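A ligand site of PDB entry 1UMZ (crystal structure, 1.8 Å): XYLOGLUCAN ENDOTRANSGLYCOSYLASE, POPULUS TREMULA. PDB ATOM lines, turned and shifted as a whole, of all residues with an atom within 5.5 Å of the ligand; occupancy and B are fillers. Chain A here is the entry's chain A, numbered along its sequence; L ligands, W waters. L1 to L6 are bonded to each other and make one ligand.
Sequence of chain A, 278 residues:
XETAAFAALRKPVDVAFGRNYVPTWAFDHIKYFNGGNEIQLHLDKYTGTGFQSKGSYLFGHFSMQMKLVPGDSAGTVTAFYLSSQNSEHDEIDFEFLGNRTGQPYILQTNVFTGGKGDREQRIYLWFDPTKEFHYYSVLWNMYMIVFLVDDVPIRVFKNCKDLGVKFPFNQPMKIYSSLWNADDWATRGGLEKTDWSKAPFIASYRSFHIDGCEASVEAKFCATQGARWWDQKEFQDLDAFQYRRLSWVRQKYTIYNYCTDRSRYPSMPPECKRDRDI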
ATOM      1  N   GLU A  91     -17.859  11.907   4.391  1.00  0.00           N
ATOM      2  CA  GLU A  91     -17.486  12.803   3.300  1.00  0.00           C
ATOM      3  C   GLU A  91     -17.613  14.252   3.732  1.00  0.00           C
ATOM      4  O   GLU A  91     -18.520  14.633   4.454  1.00  0.00           O
ATOM      5  CB  GLU A  91     -18.377  12.485   2.099  1.00  0.00           C
ATOM      6  CG  GLU A  91     -18.269  13.371   0.905  1.00  0.00           C
ATOM      7  CD  GLU A  91     -19.092  12.888  -0.284  1.00  0.00           C
ATOM      8  OE1 GLU A  91     -19.678  11.771  -0.262  1.00  0.00           O
ATOM      9  OE2 GLU A  91     -19.157  13.642  -1.246  1.00  0.00           O
ATOM     10  N   ASP A  93     -17.539  17.936   1.713  1.00  0.00           N
ATOM     11  CA  ASP A  93     -17.678  18.407   0.306  1.00  0.00           C
ATOM     12  C   ASP A  93     -17.648  19.917   0.117  1.00  0.00           C
ATOM     13  O   ASP A  93     -18.386  20.658   0.799  1.00  0.00           O
ATOM     14  CB  ASP A  93     -19.027  18.022  -0.296  1.00  0.00           C
ATOM     15  CG  ASP A  93     -19.260  16.561  -0.366  1.00  0.00           C
ATOM     16  OD1 ASP A  93     -18.382  15.802  -0.848  1.00  0.00           O
ATOM     17  OD2 ASP A  93     -20.332  16.079   0.072  1.00  0.00           O
ATOM     18  N   GLU A  95     -18.750  21.849  -3.370  1.00  0.00           N
ATOM     19  CA  GLU A  95     -19.339  21.666  -4.681  1.00  0.00           C
ATOM     20  C   GLU A  95     -19.704  23.041  -5.228  1.00  0.00           C
ATOM     21  O   GLU A  95     -20.563  23.744  -4.681  1.00  0.00           O
ATOM     22  CB  GLU A  95     -20.545  20.713  -4.644  1.00  0.00           C
ATOM     23  CG  GLU A  95     -20.099  19.289  -4.438  1.00  0.00           C
ATOM     24  CD  GLU A  95     -21.208  18.340  -4.041  1.00  0.00           C
ATOM     25  OE1 GLU A  95     -21.643  18.423  -2.854  1.00  0.00           O
ATOM     26  OE2 GLU A  95     -21.635  17.532  -4.901  1.00  0.00           O
ATOM     27  N   GLN A 108     -21.615  25.208  -2.573  1.00  0.00           N
ATOM     28  CA  GLN A 108     -22.307  24.283  -1.685  1.00  0.00           C
ATOM     29  C   GLN A 108     -21.328  23.467  -0.869  1.00  0.00           C
ATOM     30  O   GLN A 108     -20.348  22.916  -1.420  1.00  0.00           O
ATOM     31  CB  GLN A 108     -23.236  23.391  -2.462  1.00  0.00           C
ATOM     32  CG  GLN A 108     -24.069  22.444  -1.538  1.00  0.00           C
ATOM     33  CD  GLN A 108     -24.943  21.549  -2.284  1.00  0.00           C
ATOM     34  OE1 GLN A 108     -26.005  21.959  -2.724  1.00  0.00           O
ATOM     35  NE2 GLN A 108     -24.500  20.300  -2.487  1.00  0.00           N
ATOM     36  N   ASN A 110     -21.260  20.288   2.259  1.00  0.00           N
ATOM     37  CA  ASN A 110     -22.054  19.158   2.781  1.00  0.00           C
ATOM     38  C   ASN A 110     -21.142  18.288   3.625  1.00  0.00           C
ATOM     39  O   ASN A 110     -19.926  18.294   3.462  1.00  0.00           O
ATOM     40  CB  ASN A 110     -22.688  18.370   1.661  1.00  0.00           C
ATOM     41  CG  ASN A 110     -23.958  17.602   2.082  1.00  0.00           C
ATOM     42  OD1 ASN A 110     -24.326  17.583   3.263  1.00  0.00           O
ATOM     43  ND2 ASN A 110     -24.594  16.975   1.128  1.00  0.00           N
ATOM     44  N   PHE A 112     -21.220  14.239   5.113  1.00  0.00           N
ATOM     45  CA  PHE A 112     -21.801  12.913   5.329  1.00  0.00           C
ATOM     46  C   PHE A 112     -21.141  12.237   6.509  1.00  0.00           C
ATOM     47  O   PHE A 112     -19.930  12.201   6.602  1.00  0.00           O
ATOM     48  CB  PHE A 112     -21.630  12.002   4.102  1.00  0.00           C
ATOM     49  CG  PHE A 112     -22.420  12.434   2.891  1.00  0.00           C
ATOM     50  CD1 PHE A 112     -22.075  13.562   2.195  1.00  0.00           C
ATOM     51  CD2 PHE A 112     -23.496  11.678   2.433  1.00  0.00           C
ATOM     52  CE1 PHE A 112     -22.801  13.952   1.057  1.00  0.00           C
ATOM     53  CE2 PHE A 112     -24.231  12.065   1.329  1.00  0.00           C
ATOM     54  CZ  PHE A 112     -23.876  13.201   0.640  1.00  0.00           C
ATOM     55  N   ASP A 118     -27.367  15.167   3.726  1.00  0.00           N
ATOM     56  CA  ASP A 118     -28.441  16.170   3.883  1.00  0.00           C
ATOM     57  C   ASP A 118     -28.082  17.305   4.781  1.00  0.00           C
ATOM     58  O   ASP A 118     -28.899  17.796   5.570  1.00  0.00           O
ATOM     59  CB  ASP A 118     -29.737  15.507   4.375  1.00  0.00           C
ATOM     60  CG  ASP A 118     -30.125  14.377   3.513  1.00  0.00           C
ATOM     61  OD1 ASP A 118     -30.594  14.618   2.386  1.00  0.00           O
ATOM     62  OD2 ASP A 118     -29.976  13.190   3.839  1.00  0.00           O
ATOM     63  N   GLU A 120     -26.606  20.163   3.484  1.00  0.00           N
ATOM     64  CA  GLU A 120     -26.213  21.194   2.500  1.00  0.00           C
ATOM     65  C   GLU A 120     -26.271  22.609   3.064  1.00  0.00           C
ATOM     66  O   GLU A 120     -27.243  22.998   3.745  1.00  0.00           O
ATOM     67  CB  GLU A 120     -27.109  21.127   1.250  1.00  0.00           C
ATOM     68  CG  GLU A 120     -26.964  19.942   0.338  1.00  0.00           C
ATOM     69  CD  GLU A 120     -27.862  18.744   0.678  1.00  0.00           C
ATOM     70  OE1 GLU A 120     -28.420  18.689   1.791  1.00  0.00           O
ATOM     71  OE2 GLU A 120     -27.951  17.853  -0.175  1.00  0.00           O
ATOM     72  N   ARG A 122     -25.470  26.499   1.179  1.00  0.00           N
ATOM     73  CA  ARG A 122     -25.077  27.174  -0.054  1.00  0.00           C
ATOM     74  C   ARG A 122     -24.810  28.633   0.221  1.00  0.00           C
ATOM     75  O   ARG A 122     -25.615  29.341   0.872  1.00  0.00           O
ATOM     76  CB  ARG A 122     -26.176  27.054  -1.089  1.00  0.00           C
ATOM     77  CG  ARG A 122     -26.502  25.664  -1.467  1.00  0.00           C
ATOM     78  CD  ARG A 122     -27.574  25.563  -2.534  1.00  0.00           C
ATOM     79  NE  ARG A 122     -27.589  24.224  -3.032  1.00  0.00           N
ATOM     80  CZ  ARG A 122     -28.423  23.774  -3.963  1.00  0.00           C
ATOM     81  NH1 ARG A 122     -29.310  24.595  -4.492  1.00  0.00           N
ATOM     82  NH2 ARG A 122     -28.334  22.519  -4.379  1.00  0.00           N
ATOM     83  N   ASN A 181     -21.120  17.259 -15.240  1.00  0.00           N
ATOM     84  CA  ASN A 181     -22.441  17.847 -15.424  1.00  0.00           C
ATOM     85  C   ASN A 181     -23.419  17.314 -14.387  1.00  0.00           C
ATOM     86  O   ASN A 181     -23.442  16.135 -14.103  1.00  0.00           O
ATOM     87  CB  ASN A 181     -23.016  17.460 -16.797  1.00  0.00           C
ATOM     88  CG  ASN A 181     -24.479  17.867 -16.954  1.00  0.00           C
ATOM     89  OD1 ASN A 181     -25.392  17.092 -16.687  1.00  0.00           O
ATOM     90  ND2 ASN A 181     -24.696  19.086 -17.413  1.00  0.00           N
ATOM     91  N   ALA A 182     -24.247  18.210 -13.879  1.00  0.00           N
ATOM     92  CA  ALA A 182     -25.271  17.850 -12.945  1.00  0.00           C
ATOM     93  C   ALA A 182     -26.495  18.710 -13.183  1.00  0.00           C
ATOM     94  O   ALA A 182     -26.921  19.482 -12.341  1.00  0.00           O
ATOM     95  CB  ALA A 182     -24.787  18.010 -11.511  1.00  0.00           C
ATOM     96  N   ASP A 184     -29.729  18.069 -13.416  1.00  0.00           N
ATOM     97  CA  ASP A 184     -30.927  17.823 -12.617  1.00  0.00           C
ATOM     98  C   ASP A 184     -30.976  18.659 -11.339  1.00  0.00           C
ATOM     99  O   ASP A 184     -32.034  18.732 -10.722  1.00  0.00           O
ATOM    100  CB  ASP A 184     -31.063  16.331 -12.295  1.00  0.00           C
ATOM    101  CG  ASP A 184     -29.793  15.687 -11.767  1.00  0.00           C
ATOM    102  OD1 ASP A 184     -28.764  15.723 -12.473  1.00  0.00           O
ATOM    103  OD2 ASP A 184     -29.835  15.136 -10.650  1.00  0.00           O
ATOM    104  N   TRP A 185     -29.876  19.302 -10.907  1.00  0.00           N
ATOM    105  CA  TRP A 185     -29.996  20.074  -9.661  1.00  0.00           C
ATOM    106  C   TRP A 185     -29.039  21.261  -9.503  1.00  0.00           C
ATOM    107  O   TRP A 185     -29.200  22.068  -8.575  1.00  0.00           O
ATOM    108  CB  TRP A 185     -29.749  19.093  -8.471  1.00  0.00           C
ATOM    109  CG  TRP A 185     -28.367  18.497  -8.350  1.00  0.00           C
ATOM    110  CD1 TRP A 185     -27.916  17.326  -8.958  1.00  0.00           C
ATOM    111  CD2 TRP A 185     -27.230  18.969  -7.613  1.00  0.00           C
ATOM    112  NE1 TRP A 185     -26.606  17.073  -8.623  1.00  0.00           N
ATOM    113  CE2 TRP A 185     -26.162  18.062  -7.796  1.00  0.00           C
ATOM    114  CE3 TRP A 185     -27.024  20.085  -6.795  1.00  0.00           C
ATOM    115  CZ2 TRP A 185     -24.912  18.246  -7.201  1.00  0.00           C
ATOM    116  CZ3 TRP A 185     -25.790  20.244  -6.190  1.00  0.00           C
ATOM    117  CH2 TRP A 185     -24.748  19.338  -6.400  1.00  0.00           C
ATOM    118  N   GLY A 189     -31.703  25.164  -9.090  1.00  0.00           N
ATOM    119  CA  GLY A 189     -32.337  23.956  -8.589  1.00  0.00           C
ATOM    120  C   GLY A 189     -32.601  22.870  -9.647  1.00  0.00           C
ATOM    121  O   GLY A 189     -33.321  21.904  -9.377  1.00  0.00           O
ATOM    122  N   GLY A 190     -32.009  23.037 -10.820  1.00  0.00           N
ATOM    123  CA  GLY A 190     -32.158  22.097 -11.901  1.00  0.00           C
ATOM    124  C   GLY A 190     -32.855  22.710 -13.129  1.00  0.00           C
ATOM    125  O   GLY A 190     -32.943  22.087 -14.174  1.00  0.00           O
ATOM    126  N   TYR A 256     -28.866  29.181   1.428  1.00  0.00           N
ATOM    127  CA  TYR A 256     -29.511  27.958   1.873  1.00  0.00           C
ATOM    128  C   TYR A 256     -28.720  27.376   3.031  1.00  0.00           C
ATOM    129  O   TYR A 256     -27.493  27.329   3.017  1.00  0.00           O
ATOM    130  CB  TYR A 256     -29.712  26.894   0.785  1.00  0.00           C
ATOM    131  CG  TYR A 256     -30.379  25.668   1.361  1.00  0.00           C
ATOM    132  CD1 TYR A 256     -31.764  25.627   1.537  1.00  0.00           C
ATOM    133  CD2 TYR A 256     -29.630  24.568   1.838  1.00  0.00           C
ATOM    134  CE1 TYR A 256     -32.393  24.524   2.114  1.00  0.00           C
ATOM    135  CE2 TYR A 256     -30.258  23.478   2.410  1.00  0.00           C
ATOM    136  CZ  TYR A 256     -31.637  23.465   2.556  1.00  0.00           C
ATOM    137  OH  TYR A 256     -32.249  22.389   3.132  1.00  0.00           O
ATOM    138  N   ARG A 264     -37.621  20.701   5.905  1.00  0.00           N
ATOM    139  CA  ARG A 264     -36.887  19.426   5.862  1.00  0.00           C
ATOM    140  C   ARG A 264     -36.543  18.970   7.276  1.00  0.00           C
ATOM    141  O   ARG A 264     -36.554  17.791   7.590  1.00  0.00           O
ATOM    142  CB  ARG A 264     -35.585  19.572   5.027  1.00  0.00           C
ATOM    143  CG  ARG A 264     -35.552  18.746   3.729  1.00  0.00           C
ATOM    144  CD  ARG A 264     -34.178  18.114   3.354  1.00  0.00           C
ATOM    145  NE  ARG A 264     -33.094  19.094   3.302  1.00  0.00           N
ATOM    146  CZ  ARG A 264     -31.880  18.899   2.762  1.00  0.00           C
ATOM    147  NH1 ARG A 264     -31.513  17.754   2.195  1.00  0.00           N
ATOM    148  NH2 ARG A 264     -31.006  19.894   2.780  1.00  0.00           N
HETATM  149  C1  LIG L   1     -34.582  20.468  -6.355  1.00  0.00           C
HETATM  150  C2  LIG L   1     -33.275  19.660  -6.392  1.00  0.00           C
HETATM  151  C3  LIG L   1     -33.538  18.153  -6.304  1.00  0.00           C
HETATM  152  C4  LIG L   1     -34.675  17.759  -7.275  1.00  0.00           C
HETATM  153  C5  LIG L   1     -35.036  16.259  -7.213  1.00  0.00           C
HETATM  154  C6  LIG L   1     -35.635  19.934  -7.324  1.00  0.00           C
HETATM  155  O1  LIG L   1     -34.341  21.829  -6.640  1.00  0.00           O
HETATM  156  O2  LIG L   1     -32.423  20.110  -5.357  1.00  0.00           O
HETATM  157  O3  LIG L   1     -32.395  17.401  -6.716  1.00  0.00           O
HETATM  158  O4  LIG L   1     -35.827  18.558  -7.077  1.00  0.00           O
HETATM  159  O5  LIG L   1     -35.151  15.844  -5.855  1.00  0.00           O
HETATM  160  C1  LG2 L   2     -30.579  15.885  -6.243  1.00  0.00           C
HETATM  161  C2  LG2 L   2     -29.495  15.480  -5.237  1.00  0.00           C
HETATM  162  C3  LG2 L   2     -28.814  16.718  -4.655  1.00  0.00           C
HETATM  163  C4  LG2 L   2     -29.871  17.695  -4.156  1.00  0.00           C
HETATM  164  C5  LG2 L   2     -29.213  18.990  -3.712  1.00  0.00           C
HETATM  165  C6  LG2 L   2     -31.542  16.938  -5.668  1.00  0.00           C
HETATM  166  O1  LG2 L   2     -31.282  14.738  -6.677  1.00  0.00           O
HETATM  167  O2  LG2 L   2     -28.550  14.630  -5.856  1.00  0.00           O
HETATM  168  O3  LG2 L   2     -27.989  16.396  -3.535  1.00  0.00           O
HETATM  169  O4  LG2 L   2     -30.817  18.035  -5.150  1.00  0.00           O
HETATM  170  O5  LG2 L   2     -30.266  19.756  -3.154  1.00  0.00           O
HETATM  171  C1  LG3 L   3     -25.704  16.669  -2.647  1.00  0.00           C
HETATM  172  C2  LG3 L   3     -24.194  16.574  -2.968  1.00  0.00           C
HETATM  173  C3  LG3 L   3     -23.894  15.243  -3.659  1.00  0.00           C
HETATM  174  C4  LG3 L   3     -24.842  15.087  -4.852  1.00  0.00           C
HETATM  175  C5  LG3 L   3     -24.640  13.804  -5.653  1.00  0.00           C
HETATM  176  C6  LG3 L   3     -26.572  16.392  -3.875  1.00  0.00           C
HETATM  177  O1  LG3 L   3     -25.985  17.942  -2.144  1.00  0.00           O
HETATM  178  O2  LG3 L   3     -23.422  16.803  -1.803  1.00  0.00           O
HETATM  179  O3  LG3 L   3     -22.542  15.223  -4.118  1.00  0.00           O
HETATM  180  O4  LG3 L   3     -26.205  15.143  -4.444  1.00  0.00           O
HETATM  181  O5  LG3 L   3     -25.440  13.973  -6.809  1.00  0.00           O
HETATM  182  C1  LG4 L   4     -30.818  19.638  -1.484  1.00  0.00           C
HETATM  183  C2  LG4 L   4     -32.320  19.687  -1.384  1.00  0.00           C
HETATM  184  C3  LG4 L   4     -32.826  21.039  -1.896  1.00  0.00           C
HETATM  185  C4  LG4 L   4     -32.089  22.166  -1.199  1.00  0.00           C
HETATM  186  C5  LG4 L   4     -30.575  21.983  -1.296  1.00  0.00           C
HETATM  187  O1  LG4 L   4     -32.901  18.665  -2.185  1.00  0.00           O
HETATM  188  O2  LG4 L   4     -34.210  21.126  -1.640  1.00  0.00           O
HETATM  189  O3  LG4 L   4     -32.448  23.381  -1.808  1.00  0.00           O
HETATM  190  O4  LG4 L   4     -30.168  20.681  -0.894  1.00  0.00           O
HETATM  191  C1  LG5 L   5     -25.320  12.836  -7.687  1.00  0.00           C
HETATM  192  C2  LG5 L   5     -26.069  13.111  -8.968  1.00  0.00           C
HETATM  193  C3  LG5 L   5     -27.580  13.134  -8.689  1.00  0.00           C
HETATM  194  C4  LG5 L   5     -28.017  11.884  -7.931  1.00  0.00           C
HETATM  195  C5  LG5 L   5     -27.094  11.613  -6.739  1.00  0.00           C
HETATM  196  O1  LG5 L   5     -25.638  14.339  -9.529  1.00  0.00           O
HETATM  197  O2  LG5 L   5     -28.337  13.231  -9.876  1.00  0.00           O
HETATM  198  O3  LG5 L   5     -29.337  12.088  -7.466  1.00  0.00           O
HETATM  199  O4  LG5 L   5     -25.726  11.653  -7.144  1.00  0.00           O
HETATM  200  C1  LG6 L   6     -32.960  17.382  -1.514  1.00  0.00           C
HETATM  201  C2  LG6 L   6     -34.112  16.550  -2.073  1.00  0.00           C
HETATM  202  C3  LG6 L   6     -34.101  15.095  -1.590  1.00  0.00           C
HETATM  203  C4  LG6 L   6     -32.701  14.473  -1.603  1.00  0.00           C
HETATM  204  C5  LG6 L   6     -31.736  15.436  -0.927  1.00  0.00           C
HETATM  205  C6  LG6 L   6     -30.300  14.932  -0.854  1.00  0.00           C
HETATM  206  O1  LG6 L   6     -35.323  17.126  -1.672  1.00  0.00           O
HETATM  207  O2  LG6 L   6     -34.969  14.342  -2.408  1.00  0.00           O
HETATM  208  O3  LG6 L   6     -32.254  14.201  -2.919  1.00  0.00           O
HETATM  209  O4  LG6 L   6     -31.753  16.650  -1.648  1.00  0.00           O
HETATM  210  O5  LG6 L   6     -29.612  15.837  -0.021  1.00  0.00           O
HETATM  211  O   HOH W   1     -21.603  13.333  -2.547  1.00  0.00           O
HETATM  212  O   HOH W   2     -30.426  22.179  -6.262  1.00  0.00           O
HETATM  213  O   HOH W   3     -26.885  15.229   0.805  1.00  0.00           O
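O of Asn 110 lies within hydrogen-bond range of N of Asp 93 (3.0 Å).
The side-chain amide oxygen (OD1) of Asn 110 is in hydrogen-bond range of the backbone NH (N) of Glu 120 (3.5 Å).
The side-chain carboxylate of Glu 120 lies within salt-bridge range of the guanidinium group of Arg 264.
The guanidinium group of Arg 264 is in salt-bridge range of the side-chain carboxylate of Asp 118 (3.3 Å).
NH2 of Arg 264 lies within hydrogen-bond range of OH of Tyr 256 (2.8 Å).
The side-chain amide oxygen (OE1) of Gln 108 lies within hydrogen-bond range of the guanidinium group (NE) of Arg 122.
The backbone NH (N) of Arg 122 is in hydrogen-bond range of the backbone carbonyl oxygen (O) of Tyr 256, 2.9 Å away.
N of Glu 95 sits at hydrogen-bond distance from O of Gln 108, 2.7 Å away.
OD1 of Asp 118 lies within hydrogen-bond range of O5 of LG6 L6.
O1 of LG5 L5 is in hydrogen-bond range of NE1 of Trp 185 (3.0 Å).
The side-chain carboxylate of Glu 95 is in hydrogen-bond range of an oxygen (O3) of LG3 L3, at 2.6 Å.
The guanidinium group of Arg 264 sits at hydrogen-bond distance from an oxygen (O5) of LG6 L6 (3.5 Å).
The side-chain amide nitrogen of Asn 110 lies within hydrogen-bond range of an oxygen (O2) of LG3 L3 (3.2 Å).
OE2 of Glu 120 is in hydrogen-bond range of O5 of LG6 L6 (2.6 Å).
The backbone carbonyl oxygen of Gly 189 is in hydrogen-bond range of an oxygen (O1) of LIG L1, at 2.9 Å.
NE2 of Gln 108 lies within hydrogen-bond range of O1 of LG3 L3, at 2.8 Å.
The side-chain carboxylate of Asp 184 is in hydrogen-bond range of an oxygen (O2) of LG5 L5 (2.5 Å).
Merely in contact with the ligand: Asp 93 (3.7 Å), Arg 122 (3.6 Å) and Tyr 256 (3.999 Å).
Hydrophobic or aromatic side chains that line the ligand: Trp 185 and Tyr 256.
Within 4 Å of the ligand: Asp 93, Glu 95, Gln 108, Asn 110, Asp 118, Glu 120, Arg 122, Asp 184, Trp 185, Gly 189, Tyr 256 and Arg 264.
Water W1 bridges an oxygen (O3) of LG3 L3 and the side-chain carboxylate of Glu 91.
Water W3 lies within hydrogen-bond range of ND2 of Asn 110, O5 of LG6 L6, N of Asp 118 and OE2 of Glu 120.
Water W2 lies within hydrogen-bond range of the backbone carbonyl oxygen of Trp 185, the guanidinium group of Arg 122 and an oxygen (O2) of LIG L1.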
